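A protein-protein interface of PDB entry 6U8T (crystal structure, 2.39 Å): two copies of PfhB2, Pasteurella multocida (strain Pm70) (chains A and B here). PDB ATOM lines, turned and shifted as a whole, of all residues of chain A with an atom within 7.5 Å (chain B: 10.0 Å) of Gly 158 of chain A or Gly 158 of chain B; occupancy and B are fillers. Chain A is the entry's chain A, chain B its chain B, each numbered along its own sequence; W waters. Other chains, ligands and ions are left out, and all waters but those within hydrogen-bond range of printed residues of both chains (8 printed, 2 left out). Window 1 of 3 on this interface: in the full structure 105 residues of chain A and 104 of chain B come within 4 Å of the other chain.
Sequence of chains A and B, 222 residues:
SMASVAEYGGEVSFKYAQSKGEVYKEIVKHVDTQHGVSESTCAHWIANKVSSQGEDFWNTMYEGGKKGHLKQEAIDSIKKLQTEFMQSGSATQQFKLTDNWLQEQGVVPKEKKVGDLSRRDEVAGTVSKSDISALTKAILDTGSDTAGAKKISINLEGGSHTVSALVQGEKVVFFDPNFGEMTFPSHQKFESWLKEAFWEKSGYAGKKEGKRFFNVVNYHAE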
ATOM      1  N   TYR A  24      12.055  12.929 -21.505  1.00  0.00           N
ATOM      2  CA  TYR A  24      10.601  12.702 -21.748  1.00  0.00           C
ATOM      3  C   TYR A  24       9.971  12.005 -20.532  1.00  0.00           C
ATOM      4  O   TYR A  24       8.852  12.362 -20.157  1.00  0.00           O
ATOM      5  CB  TYR A  24      10.316  11.965 -23.063  1.00  0.00           C
ATOM      6  CG  TYR A  24       8.827  11.822 -23.282  1.00  0.00           C
ATOM      7  CD1 TYR A  24       8.038  12.935 -23.524  1.00  0.00           C
ATOM      8  CD2 TYR A  24       8.182  10.615 -23.070  1.00  0.00           C
ATOM      9  CE1 TYR A  24       6.663  12.838 -23.646  1.00  0.00           C
ATOM     10  CE2 TYR A  24       6.805  10.503 -23.191  1.00  0.00           C
ATOM     11  CZ  TYR A  24       6.050  11.613 -23.523  1.00  0.00           C
ATOM     12  OH  TYR A  24       4.690  11.546 -23.658  1.00  0.00           O
ATOM     13  N   VAL A  31       4.055  16.133 -15.328  1.00  0.00           N
ATOM     14  CA  VAL A  31       2.640  16.332 -15.766  1.00  0.00           C
ATOM     15  C   VAL A  31       1.705  15.432 -14.940  1.00  0.00           C
ATOM     16  O   VAL A  31       0.653  15.885 -14.546  1.00  0.00           O
ATOM     17  CB  VAL A  31       2.505  16.080 -17.274  1.00  0.00           C
ATOM     18  CG1 VAL A  31       1.061  16.010 -17.687  1.00  0.00           C
ATOM     19  CG2 VAL A  31       3.256  17.118 -18.094  1.00  0.00           C
ATOM     20  N   ASN A 155      -8.556  16.298 -20.902  1.00  0.00           N
ATOM     21  CA  ASN A 155      -7.404  15.517 -21.422  1.00  0.00           C
ATOM     22  C   ASN A 155      -6.582  16.474 -22.285  1.00  0.00           C
ATOM     23  O   ASN A 155      -7.175  17.302 -22.980  1.00  0.00           O
ATOM     24  CB  ASN A 155      -7.878  14.227 -22.105  1.00  0.00           C
ATOM     25  CG  ASN A 155      -7.979  13.063 -21.134  1.00  0.00           C
ATOM     26  OD1 ASN A 155      -8.363  11.932 -21.508  1.00  0.00           O
ATOM     27  ND2 ASN A 155      -7.544  13.287 -19.905  1.00  0.00           N
ATOM     28  N   LEU A 156      -5.272  16.405 -22.166  1.00  0.00           N
ATOM     29  CA  LEU A 156      -4.332  17.269 -22.932  1.00  0.00           C
ATOM     30  C   LEU A 156      -3.759  16.461 -24.119  1.00  0.00           C
ATOM     31  O   LEU A 156      -3.753  15.218 -24.077  1.00  0.00           O
ATOM     32  CB  LEU A 156      -3.218  17.741 -21.996  1.00  0.00           C
ATOM     33  CG  LEU A 156      -3.675  18.422 -20.707  1.00  0.00           C
ATOM     34  CD1 LEU A 156      -2.509  18.554 -19.738  1.00  0.00           C
ATOM     35  CD2 LEU A 156      -4.307  19.780 -20.980  1.00  0.00           C
ATOM     36  N   GLU A 157      -3.353  17.163 -25.159  1.00  0.00           N
ATOM     37  CA  GLU A 157      -2.735  16.597 -26.370  1.00  0.00           C
ATOM     38  C   GLU A 157      -1.392  15.997 -25.988  1.00  0.00           C
ATOM     39  O   GLU A 157      -0.631  16.667 -25.327  1.00  0.00           O
ATOM     40  CB  GLU A 157      -2.558  17.671 -27.435  1.00  0.00           C
ATOM     41  CG  GLU A 157      -2.271  17.077 -28.790  1.00  0.00           C
ATOM     42  CD  GLU A 157      -2.367  18.123 -29.874  1.00  0.00           C
ATOM     43  OE1 GLU A 157      -1.521  19.048 -29.865  1.00  0.00           O
ATOM     44  OE2 GLU A 157      -3.295  18.010 -30.691  1.00  0.00           O
ATOM     45  N   GLY A 158      -1.187  14.728 -26.320  1.00  0.00           N
ATOM     46  CA  GLY A 158       0.115  14.073 -26.225  1.00  0.00           C
ATOM     47  C   GLY A 158       0.965  14.516 -27.394  1.00  0.00           C
ATOM     48  O   GLY A 158       0.425  15.000 -28.398  1.00  0.00           O
ATOM     49  N   GLY A 159       2.269  14.382 -27.247  1.00  0.00           N
ATOM     50  CA  GLY A 159       3.199  14.730 -28.333  1.00  0.00           C
ATOM     51  C   GLY A 159       3.264  13.646 -29.409  1.00  0.00           C
ATOM     52  O   GLY A 159       2.548  12.600 -29.319  1.00  0.00           O
ATOM     53  N   SER A 160       4.137  13.885 -30.378  1.00  0.00           N
ATOM     54  CA  SER A 160       4.471  12.932 -31.458  1.00  0.00           C
ATOM     55  C   SER A 160       5.943  12.534 -31.373  1.00  0.00           C
ATOM     56  O   SER A 160       6.758  13.340 -30.943  1.00  0.00           O
ATOM     57  CB  SER A 160       4.131  13.531 -32.763  1.00  0.00           C
ATOM     58  OG  SER A 160       2.736  13.727 -32.797  1.00  0.00           O
ATOM     59  N   GLY A 206       1.964   4.660 -21.910  1.00  0.00           N
ATOM     60  CA  GLY A 206       0.973   5.503 -21.211  1.00  0.00           C
ATOM     61  C   GLY A 206       0.507   4.818 -19.937  1.00  0.00           C
ATOM     62  O   GLY A 206       0.955   3.682 -19.705  1.00  0.00           O
ATOM     63  N   LYS A 207      -0.362   5.453 -19.150  1.00  0.00           N
ATOM     64  CA  LYS A 207      -0.922   4.891 -17.886  1.00  0.00           C
ATOM     65  C   LYS A 207      -2.327   4.338 -18.153  1.00  0.00           C
ATOM     66  O   LYS A 207      -2.735   3.377 -17.501  1.00  0.00           O
ATOM     67  CB  LYS A 207      -0.977   5.955 -16.787  1.00  0.00           C
ATOM     68  CG  LYS A 207       0.373   6.458 -16.304  1.00  0.00           C
ATOM     69  CD  LYS A 207       0.798   7.746 -16.965  1.00  0.00           C
ATOM     70  CE  LYS A 207       1.905   8.471 -16.219  1.00  0.00           C
ATOM     71  NZ  LYS A 207       3.082   7.598 -15.975  1.00  0.00           N
ATOM     72  N   LYS A 208      -3.071   4.979 -19.044  1.00  0.00           N
ATOM     73  CA  LYS A 208      -4.506   4.698 -19.285  1.00  0.00           C
ATOM     74  C   LYS A 208      -4.593   3.699 -20.437  1.00  0.00           C
ATOM     75  O   LYS A 208      -3.586   3.511 -21.152  1.00  0.00           O
ATOM     76  CB  LYS A 208      -5.263   6.000 -19.564  1.00  0.00           C
ATOM     77  CG  LYS A 208      -5.178   7.005 -18.435  1.00  0.00           C
ATOM     78  CD  LYS A 208      -6.040   8.210 -18.634  1.00  0.00           C
ATOM     79  CE  LYS A 208      -5.472   9.254 -19.569  1.00  0.00           C
ATOM     80  NZ  LYS A 208      -6.067  10.579 -19.261  1.00  0.00           N
ATOM     81  N   ARG A 212      -4.136   4.950 -29.634  1.00  0.00           N
ATOM     82  CA  ARG A 212      -3.404   6.103 -30.238  1.00  0.00           C
ATOM     83  C   ARG A 212      -2.946   5.638 -31.618  1.00  0.00           C
ATOM     84  O   ARG A 212      -2.672   4.446 -31.749  1.00  0.00           O
ATOM     85  CB  ARG A 212      -2.234   6.554 -29.359  1.00  0.00           C
ATOM     86  CG  ARG A 212      -2.633   6.905 -27.933  1.00  0.00           C
ATOM     87  CD  ARG A 212      -1.454   7.424 -27.148  1.00  0.00           C
ATOM     88  NE  ARG A 212      -0.519   6.362 -26.852  1.00  0.00           N
ATOM     89  CZ  ARG A 212      -0.706   5.403 -25.947  1.00  0.00           C
ATOM     90  NH1 ARG A 212      -1.814   5.361 -25.195  1.00  0.00           N
ATOM     91  NH2 ARG A 212       0.233   4.485 -25.790  1.00  0.00           N
ATOM     92  N   TYR B  24       3.996  24.247 -18.084  1.00  0.00           N
ATOM     93  CA  TYR B  24       3.348  23.307 -19.029  1.00  0.00           C
ATOM     94  C   TYR B  24       3.542  23.794 -20.482  1.00  0.00           C
ATOM     95  O   TYR B  24       3.780  22.968 -21.372  1.00  0.00           O
ATOM     96  CB  TYR B  24       1.876  23.027 -18.667  1.00  0.00           C
ATOM     97  CG  TYR B  24       1.273  22.034 -19.617  1.00  0.00           C
ATOM     98  CD1 TYR B  24       1.667  20.715 -19.570  1.00  0.00           C
ATOM     99  CD2 TYR B  24       0.453  22.422 -20.656  1.00  0.00           C
ATOM    100  CE1 TYR B  24       1.145  19.771 -20.441  1.00  0.00           C
ATOM    101  CE2 TYR B  24      -0.003  21.514 -21.594  1.00  0.00           C
ATOM    102  CZ  TYR B  24       0.334  20.183 -21.484  1.00  0.00           C
ATOM    103  OH  TYR B  24      -0.154  19.291 -22.408  1.00  0.00           O
ATOM    104  N   ILE B  27       6.953  22.864 -21.632  1.00  0.00           N
ATOM    105  CA  ILE B  27       6.958  21.394 -21.894  1.00  0.00           C
ATOM    106  C   ILE B  27       6.384  21.135 -23.292  1.00  0.00           C
ATOM    107  O   ILE B  27       6.992  20.381 -24.086  1.00  0.00           O
ATOM    108  CB  ILE B  27       6.202  20.652 -20.789  1.00  0.00           C
ATOM    109  CG1 ILE B  27       6.948  20.703 -19.454  1.00  0.00           C
ATOM    110  CG2 ILE B  27       5.933  19.229 -21.214  1.00  0.00           C
ATOM    111  CD1 ILE B  27       6.155  20.162 -18.255  1.00  0.00           C
ATOM    112  N   VAL B  28       5.257  21.754 -23.620  1.00  0.00           N
ATOM    113  CA  VAL B  28       4.606  21.594 -24.954  1.00  0.00           C
ATOM    114  C   VAL B  28       5.595  22.029 -26.044  1.00  0.00           C
ATOM    115  O   VAL B  28       5.753  21.291 -27.028  1.00  0.00           O
ATOM    116  CB  VAL B  28       3.274  22.366 -25.027  1.00  0.00           C
ATOM    117  CG1 VAL B  28       2.781  22.522 -26.456  1.00  0.00           C
ATOM    118  CG2 VAL B  28       2.200  21.711 -24.159  1.00  0.00           C
ATOM    119  N   VAL B  31       8.406  19.260 -26.361  1.00  0.00           N
ATOM    120  CA  VAL B  31       7.890  18.008 -26.987  1.00  0.00           C
ATOM    121  C   VAL B  31       7.614  18.250 -28.485  1.00  0.00           C
ATOM    122  O   VAL B  31       7.924  17.382 -29.299  1.00  0.00           O
ATOM    123  CB  VAL B  31       6.631  17.519 -26.249  1.00  0.00           C
ATOM    124  CG1 VAL B  31       5.947  16.427 -27.019  1.00  0.00           C
ATOM    125  CG2 VAL B  31       6.961  17.035 -24.850  1.00  0.00           C
ATOM    126  N   ASP B  32       7.072  19.415 -28.847  1.00  0.00           N
ATOM    127  CA  ASP B  32       6.860  19.787 -30.271  1.00  0.00           C
ATOM    128  C   ASP B  32       8.221  19.861 -30.986  1.00  0.00           C
ATOM    129  O   ASP B  32       8.355  19.232 -32.044  1.00  0.00           O
ATOM    130  CB  ASP B  32       6.084  21.099 -30.376  1.00  0.00           C
ATOM    131  CG  ASP B  32       5.460  21.308 -31.749  1.00  0.00           C
ATOM    132  OD1 ASP B  32       4.743  20.416 -32.225  1.00  0.00           O
ATOM    133  OD2 ASP B  32       5.708  22.358 -32.345  1.00  0.00           O
ATOM    134  N   HIS B  35       9.895  16.500 -31.532  1.00  0.00           N
ATOM    135  CA  HIS B  35       9.288  15.778 -32.674  1.00  0.00           C
ATOM    136  C   HIS B  35      10.075  16.119 -33.955  1.00  0.00           C
ATOM    137  O   HIS B  35      10.451  15.199 -34.700  1.00  0.00           O
ATOM    138  CB  HIS B  35       7.779  16.026 -32.764  1.00  0.00           C
ATOM    139  CG  HIS B  35       7.146  15.277 -33.891  1.00  0.00           C
ATOM    140  ND1 HIS B  35       6.152  15.819 -34.672  1.00  0.00           N
ATOM    141  CD2 HIS B  35       7.434  14.064 -34.434  1.00  0.00           C
ATOM    142  CE1 HIS B  35       5.799  14.958 -35.597  1.00  0.00           C
ATOM    143  NE2 HIS B  35       6.565  13.873 -35.480  1.00  0.00           N
ATOM    144  N   ILE B 154       4.654   7.583 -33.918  1.00  0.00           N
ATOM    145  CA  ILE B 154       3.827   7.133 -32.776  1.00  0.00           C
ATOM    146  C   ILE B 154       3.299   8.354 -32.042  1.00  0.00           C
ATOM    147  O   ILE B 154       4.040   9.348 -31.880  1.00  0.00           O
ATOM    148  CB  ILE B 154       4.560   6.168 -31.840  1.00  0.00           C
ATOM    149  CG1 ILE B 154       5.627   6.855 -31.009  1.00  0.00           C
ATOM    150  CG2 ILE B 154       5.132   4.984 -32.612  1.00  0.00           C
ATOM    151  CD1 ILE B 154       6.379   5.882 -30.142  1.00  0.00           C
ATOM    152  N   ASN B 155       2.022   8.299 -31.692  1.00  0.00           N
ATOM    153  CA  ASN B 155       1.337   9.350 -30.897  1.00  0.00           C
ATOM    154  C   ASN B 155       1.473   8.961 -29.434  1.00  0.00           C
ATOM    155  O   ASN B 155       1.423   7.790 -29.128  1.00  0.00           O
ATOM    156  CB  ASN B 155      -0.064   9.584 -31.436  1.00  0.00           C
ATOM    157  CG  ASN B 155       0.048  10.170 -32.825  1.00  0.00           C
ATOM    158  OD1 ASN B 155       0.617  11.231 -33.007  1.00  0.00           O
ATOM    159  ND2 ASN B 155      -0.283   9.392 -33.827  1.00  0.00           N
ATOM    160  N   LEU B 156       1.744   9.939 -28.585  1.00  0.00           N
ATOM    161  CA  LEU B 156       1.997   9.749 -27.141  1.00  0.00           C
ATOM    162  C   LEU B 156       0.734  10.107 -26.357  1.00  0.00           C
ATOM    163  O   LEU B 156      -0.137  10.879 -26.866  1.00  0.00           O
ATOM    164  CB  LEU B 156       3.166  10.656 -26.755  1.00  0.00           C
ATOM    165  CG  LEU B 156       4.495  10.348 -27.449  1.00  0.00           C
ATOM    166  CD1 LEU B 156       5.514  11.387 -27.057  1.00  0.00           C
ATOM    167  CD2 LEU B 156       5.052   8.993 -27.091  1.00  0.00           C
ATOM    168  N   GLU B 157       0.643   9.542 -25.154  1.00  0.00           N
ATOM    169  CA  GLU B 157      -0.435   9.833 -24.195  1.00  0.00           C
ATOM    170  C   GLU B 157      -0.277  11.287 -23.753  1.00  0.00           C
ATOM    171  O   GLU B 157       0.808  11.654 -23.399  1.00  0.00           O
ATOM    172  CB  GLU B 157      -0.372   8.873 -23.014  1.00  0.00           C
ATOM    173  CG  GLU B 157      -1.642   8.929 -22.183  1.00  0.00           C
ATOM    174  CD  GLU B 157      -1.696   7.834 -21.150  1.00  0.00           C
ATOM    175  OE1 GLU B 157      -0.883   7.942 -20.205  1.00  0.00           O
ATOM    176  OE2 GLU B 157      -2.499   6.854 -21.340  1.00  0.00           O
ATOM    177  N   GLY B 158      -1.333  12.078 -23.848  1.00  0.00           N
ATOM    178  CA  GLY B 158      -1.402  13.396 -23.227  1.00  0.00           C
ATOM    179  C   GLY B 158      -1.620  13.225 -21.740  1.00  0.00           C
ATOM    180  O   GLY B 158      -2.120  12.159 -21.320  1.00  0.00           O
ATOM    181  N   GLY B 159      -1.246  14.216 -20.944  1.00  0.00           N
ATOM    182  CA  GLY B 159      -1.623  14.212 -19.521  1.00  0.00           C
ATOM    183  C   GLY B 159      -3.086  14.565 -19.289  1.00  0.00           C
ATOM    184  O   GLY B 159      -3.859  14.770 -20.254  1.00  0.00           O
ATOM    185  N   SER B 160      -3.434  14.665 -18.018  1.00  0.00           N
ATOM    186  CA  SER B 160      -4.773  15.085 -17.543  1.00  0.00           C
ATOM    187  C   SER B 160      -4.636  16.362 -16.712  1.00  0.00           C
ATOM    188  O   SER B 160      -3.586  16.554 -16.064  1.00  0.00           O
ATOM    189  CB  SER B 160      -5.385  13.980 -16.784  1.00  0.00           C
ATOM    190  OG  SER B 160      -5.498  12.827 -17.614  1.00  0.00           O
ATOM    191  N   HIS B 161      -5.644  17.223 -16.773  1.00  0.00           N
ATOM    192  CA  HIS B 161      -5.707  18.464 -15.970  1.00  0.00           C
ATOM    193  C   HIS B 161      -7.104  18.559 -15.361  1.00  0.00           C
ATOM    194  O   HIS B 161      -8.066  18.038 -15.970  1.00  0.00           O
ATOM    195  CB  HIS B 161      -5.338  19.674 -16.830  1.00  0.00           C
ATOM    196  CG  HIS B 161      -5.222  20.926 -16.045  1.00  0.00           C
ATOM    197  ND1 HIS B 161      -4.500  20.991 -14.876  1.00  0.00           N
ATOM    198  CD2 HIS B 161      -5.713  22.163 -16.263  1.00  0.00           C
ATOM    199  CE1 HIS B 161      -4.544  22.217 -14.399  1.00  0.00           C
ATOM    200  NE2 HIS B 161      -5.280  22.966 -15.235  1.00  0.00           N
ATOM    201  N   GLY B 203      -2.372  26.563 -23.609  1.00  0.00           N
ATOM    202  CA  GLY B 203      -1.677  25.353 -24.089  1.00  0.00           C
ATOM    203  C   GLY B 203      -2.571  24.116 -24.105  1.00  0.00           C
ATOM    204  O   GLY B 203      -2.077  23.049 -24.501  1.00  0.00           O
ATOM    205  N   TYR B 204      -3.829  24.208 -23.672  1.00  0.00           N
ATOM    206  CA  TYR B 204      -4.747  23.040 -23.574  1.00  0.00           C
ATOM    207  C   TYR B 204      -5.337  22.699 -24.957  1.00  0.00           C
ATOM    208  O   TYR B 204      -5.846  21.585 -25.114  1.00  0.00           O
ATOM    209  CB  TYR B 204      -5.855  23.292 -22.541  1.00  0.00           C
ATOM    210  CG  TYR B 204      -5.416  23.678 -21.153  1.00  0.00           C
ATOM    211  CD1 TYR B 204      -4.195  23.295 -20.613  1.00  0.00           C
ATOM    212  CD2 TYR B 204      -6.246  24.450 -20.354  1.00  0.00           C
ATOM    213  CE1 TYR B 204      -3.811  23.679 -19.330  1.00  0.00           C
ATOM    214  CE2 TYR B 204      -5.882  24.839 -19.072  1.00  0.00           C
ATOM    215  CZ  TYR B 204      -4.664  24.441 -18.553  1.00  0.00           C
ATOM    216  OH  TYR B 204      -4.292  24.792 -17.299  1.00  0.00           O
ATOM    217  N   ALA B 205      -5.335  23.632 -25.911  1.00  0.00           N
ATOM    218  CA  ALA B 205      -6.022  23.464 -27.219  1.00  0.00           C
ATOM    219  C   ALA B 205      -5.308  22.385 -28.044  1.00  0.00           C
ATOM    220  O   ALA B 205      -6.016  21.510 -28.609  1.00  0.00           O
ATOM    221  CB  ALA B 205      -6.078  24.759 -27.979  1.00  0.00           C
ATOM    222  N   GLY B 206      -3.973  22.444 -28.089  1.00  0.00           N
ATOM    223  CA  GLY B 206      -3.116  21.510 -28.842  1.00  0.00           C
ATOM    224  C   GLY B 206      -2.836  22.060 -30.227  1.00  0.00           C
ATOM    225  O   GLY B 206      -3.407  23.116 -30.557  1.00  0.00           O
ATOM    226  N   LYS B 207      -1.968  21.397 -31.005  1.00  0.00           N
ATOM    227  CA  LYS B 207      -1.626  21.793 -32.397  1.00  0.00           C
ATOM    228  C   LYS B 207      -2.419  20.943 -33.386  1.00  0.00           C
ATOM    229  O   LYS B 207      -2.794  21.478 -34.447  1.00  0.00           O
ATOM    230  CB  LYS B 207      -0.124  21.649 -32.634  1.00  0.00           C
ATOM    231  CG  LYS B 207       0.718  22.670 -31.884  1.00  0.00           C
ATOM    232  CD  LYS B 207       1.238  22.224 -30.524  1.00  0.00           C
ATOM    233  CE  LYS B 207       1.386  23.378 -29.547  1.00  0.00           C
ATOM    234  NZ  LYS B 207       2.095  24.538 -30.141  1.00  0.00           N
ATOM    235  N   LYS B 208      -2.651  19.679 -33.052  1.00  0.00           N
ATOM    236  CA  LYS B 208      -3.226  18.665 -33.970  1.00  0.00           C
ATOM    237  C   LYS B 208      -4.749  18.681 -33.833  1.00  0.00           C
ATOM    238  O   LYS B 208      -5.258  19.281 -32.865  1.00  0.00           O
ATOM    239  CB  LYS B 208      -2.661  17.279 -33.655  1.00  0.00           C
ATOM    240  CG  LYS B 208      -1.144  17.181 -33.674  1.00  0.00           C
ATOM    241  CD  LYS B 208      -0.603  15.978 -32.926  1.00  0.00           C
ATOM    242  CE  LYS B 208      -0.857  14.617 -33.564  1.00  0.00           C
ATOM    243  NZ  LYS B 208      -0.889  14.638 -35.052  1.00  0.00           N
ATOM    244  N   GLU B 209      -5.433  18.113 -34.824  1.00  0.00           N
ATOM    245  CA  GLU B 209      -6.878  17.794 -34.739  1.00  0.00           C
ATOM    246  C   GLU B 209      -6.979  16.482 -33.968  1.00  0.00           C
ATOM    247  O   GLU B 209      -5.976  15.760 -33.915  1.00  0.00           O
ATOM    248  CB  GLU B 209      -7.516  17.745 -36.128  1.00  0.00           C
ATOM    249  CG  GLU B 209      -7.627  19.116 -36.769  1.00  0.00           C
ATOM    250  CD  GLU B 209      -8.439  20.141 -35.990  1.00  0.00           C
ATOM    251  OE1 GLU B 209      -9.253  19.728 -35.132  1.00  0.00           O
ATOM    252  OE2 GLU B 209      -8.233  21.351 -36.223  1.00  0.00           O
ATOM    253  N   GLY B 210      -8.106  16.233 -33.322  1.00  0.00           N
ATOM    254  CA  GLY B 210      -8.235  15.076 -32.426  1.00  0.00           C
ATOM    255  C   GLY B 210      -9.161  15.398 -31.290  1.00  0.00           C
ATOM    256  O   GLY B 210      -8.985  16.466 -30.677  1.00  0.00           O
ATOM    257  N   LYS B 211     -10.111  14.503 -31.026  1.00  0.00           N
ATOM    258  CA  LYS B 211     -11.071  14.618 -29.902  1.00  0.00           C
ATOM    259  C   LYS B 211     -10.383  14.103 -28.636  1.00  0.00           C
ATOM    260  O   LYS B 211      -9.704  13.055 -28.713  1.00  0.00           O
ATOM    261  CB  LYS B 211     -12.345  13.856 -30.244  1.00  0.00           C
ATOM    262  CG  LYS B 211     -12.979  14.243 -31.572  1.00  0.00           C
ATOM    263  CD  LYS B 211     -13.210  15.730 -31.733  1.00  0.00           C
ATOM    264  CE  LYS B 211     -14.285  16.053 -32.743  1.00  0.00           C
ATOM    265  NZ  LYS B 211     -14.710  17.466 -32.608  1.00  0.00           N
ATOM    266  N   ARG B 212     -10.493  14.856 -27.539  1.00  0.00           N
ATOM    267  CA  ARG B 212      -9.946  14.477 -26.216  1.00  0.00           C
ATOM    268  C   ARG B 212     -11.123  14.501 -25.246  1.00  0.00           C
ATOM    269  O   ARG B 212     -12.035  15.306 -25.458  1.00  0.00           O
ATOM    270  CB  ARG B 212      -8.827  15.433 -25.802  1.00  0.00           C
ATOM    271  CG  ARG B 212      -7.654  15.464 -26.770  1.00  0.00           C
ATOM    272  CD  ARG B 212      -6.488  16.231 -26.196  1.00  0.00           C
ATOM    273  NE  ARG B 212      -6.790  17.656 -26.116  1.00  0.00           N
ATOM    274  CZ  ARG B 212      -6.826  18.482 -27.157  1.00  0.00           C
ATOM    275  NH1 ARG B 212      -6.593  18.060 -28.392  1.00  0.00           N
ATOM    276  NH2 ARG B 212      -7.124  19.742 -26.964  1.00  0.00           N
ATOM    277  N   PHE B 213     -11.103  13.631 -24.243  1.00  0.00           N
ATOM    278  CA  PHE B 213     -12.201  13.457 -23.262  1.00  0.00           C
ATOM    279  C   PHE B 213     -12.170  14.608 -22.259  1.00  0.00           C
ATOM    280  O   PHE B 213     -11.110  15.157 -21.920  1.00  0.00           O
ATOM    281  CB  PHE B 213     -12.086  12.107 -22.564  1.00  0.00           C
ATOM    282  CG  PHE B 213     -12.261  10.923 -23.477  1.00  0.00           C
ATOM    283  CD1 PHE B 213     -13.342  10.849 -24.343  1.00  0.00           C
ATOM    284  CD2 PHE B 213     -11.333   9.887 -23.480  1.00  0.00           C
ATOM    285  CE1 PHE B 213     -13.521   9.736 -25.161  1.00  0.00           C
ATOM    286  CE2 PHE B 213     -11.522   8.785 -24.295  1.00  0.00           C
ATOM    287  CZ  PHE B 213     -12.604   8.718 -25.143  1.00  0.00           C
HETATM  288  O   HOH W   1       5.007  16.711 -30.545  1.00  0.00           O
HETATM  289  O   HOH W   2       0.039  16.800 -21.992  1.00  0.00           O
HETATM  290  O   HOH W   3      -1.031  12.117 -29.166  1.00  0.00           O
HETATM  291  O   HOH W   4      -4.069   6.748 -23.339  1.00  0.00           O
HETATM  292  O   HOH W   5       8.398  14.635 -29.012  1.00  0.00           O
HETATM  293  O   HOH W   6      -8.581  11.760 -24.321  1.00  0.00           O
HETATM  294  O   HOH W   7       3.041  13.464 -24.394  1.00  0.00           O
HETATM  295  O   HOH W   8       2.004   5.419 -28.012  1.00  0.00           O
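The side-chain hydroxyl (OG) of Ser 160 of chain B is in hydrogen-bond range of the side-chain amino group (NZ) of Lys 208 of chain A (2.8 Å). OD1 of Asn 155 of chain B sits at hydrogen-bond distance from OG of Ser 160 of chain A (3.3 Å). NE of Arg 212 of chain A lies within hydrogen-bond range of O of Asn 155 of chain B. O of Gly 159 of chain A sits at hydrogen-bond distance from N of Leu 156 of chain B (2.9 Å). OE1 of Glu 157 of chain A lies within hydrogen-bond range of N of Lys 207 of chain B. N of Lys 207 of chain A sits at hydrogen-bond distance from OE1 of Glu 157 of chain B (2.8 Å). The side-chain carboxylate (OE2) of Glu 157 of chain A lies within hydrogen-bond range of the backbone NH (N) of Lys 208 of chain B. The guanidinium group of Arg 212 of chain B sits at hydrogen-bond distance from the backbone carbonyl oxygen of Asn 155 of chain A (3.2 Å). N of Leu 156 of chain A sits at hydrogen-bond distance from O of Gly 159 of chain B (2.9 Å). The backbone NH (N) of Lys 208 of chain A sits at hydrogen-bond distance from the side-chain carboxylate (OE2) of Glu 157 of chain B (3.0 Å). The side-chain hydroxyl (OG) of Ser 160 of chain B is in hydrogen-bond range of the side-chain amide nitrogen (ND2) of Asn 155 of chain A (3.1 Å). The backbone NH of Asn 155 of chain A sits at hydrogen-bond distance from the backbone carbonyl oxygen of Phe 213 of chain B (3.0 Å).
The side-chain hydroxyl of Tyr 204 of chain B sits at hydrogen-bond distance from a ring nitrogen (NE2) of His 161 of chain B, at 2.9 Å.
Of the printed residues of chain B, Gly 158 of chain A touches Leu 156 (3.3 Å), Glu 157 (3.7 Å) and Gly 158 (3.4 Å). Of chain B, only Val 31 (3.5 Å), Asn 155 (3.8 Å) and Leu 156 (2.9 Å) come within 4 Å of Gly 159 of chain A. Gly 159 of chain B touches three residues of chain A. Asp 32 of chain B touches none of the printed residues of chain A. The nearest residue of chain B that does not touch Gly 158 of chain A is Lys 208 of chain B (4.7 Å).
Of the 12 printed residues of chain A, 12 touch a printed residue of chain B. Hydrophobic or aromatic side chains of chain A within 4 Å of the printed part of chain B: Tyr 24, Val 31 and Leu 156. Of the 25 printed residues of chain B, 16 touch a printed residue of chain A. Among the printed residues, 35 pairs touch across the chains. Among the printed residues, no Asp or Glu carboxylate lies within 4 Å of a Lys or Arg side-chain nitrogen of the other chain.
Glu 157 of chain A touches Lys 207 of chain B, and with the chains exchanged Lys 207 of chain A touches Glu 157 of chain B. 12 positions are printed for both chains.
Water W7 lies within hydrogen-bond range of the side-chain hydroxyl of Tyr 24 of chain A (2.6 Å), the backbone carbonyl oxygen of Glu 157 of chain B (3.0 Å) and the backbone NH of Gly 159 of chain A (3.1 Å).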
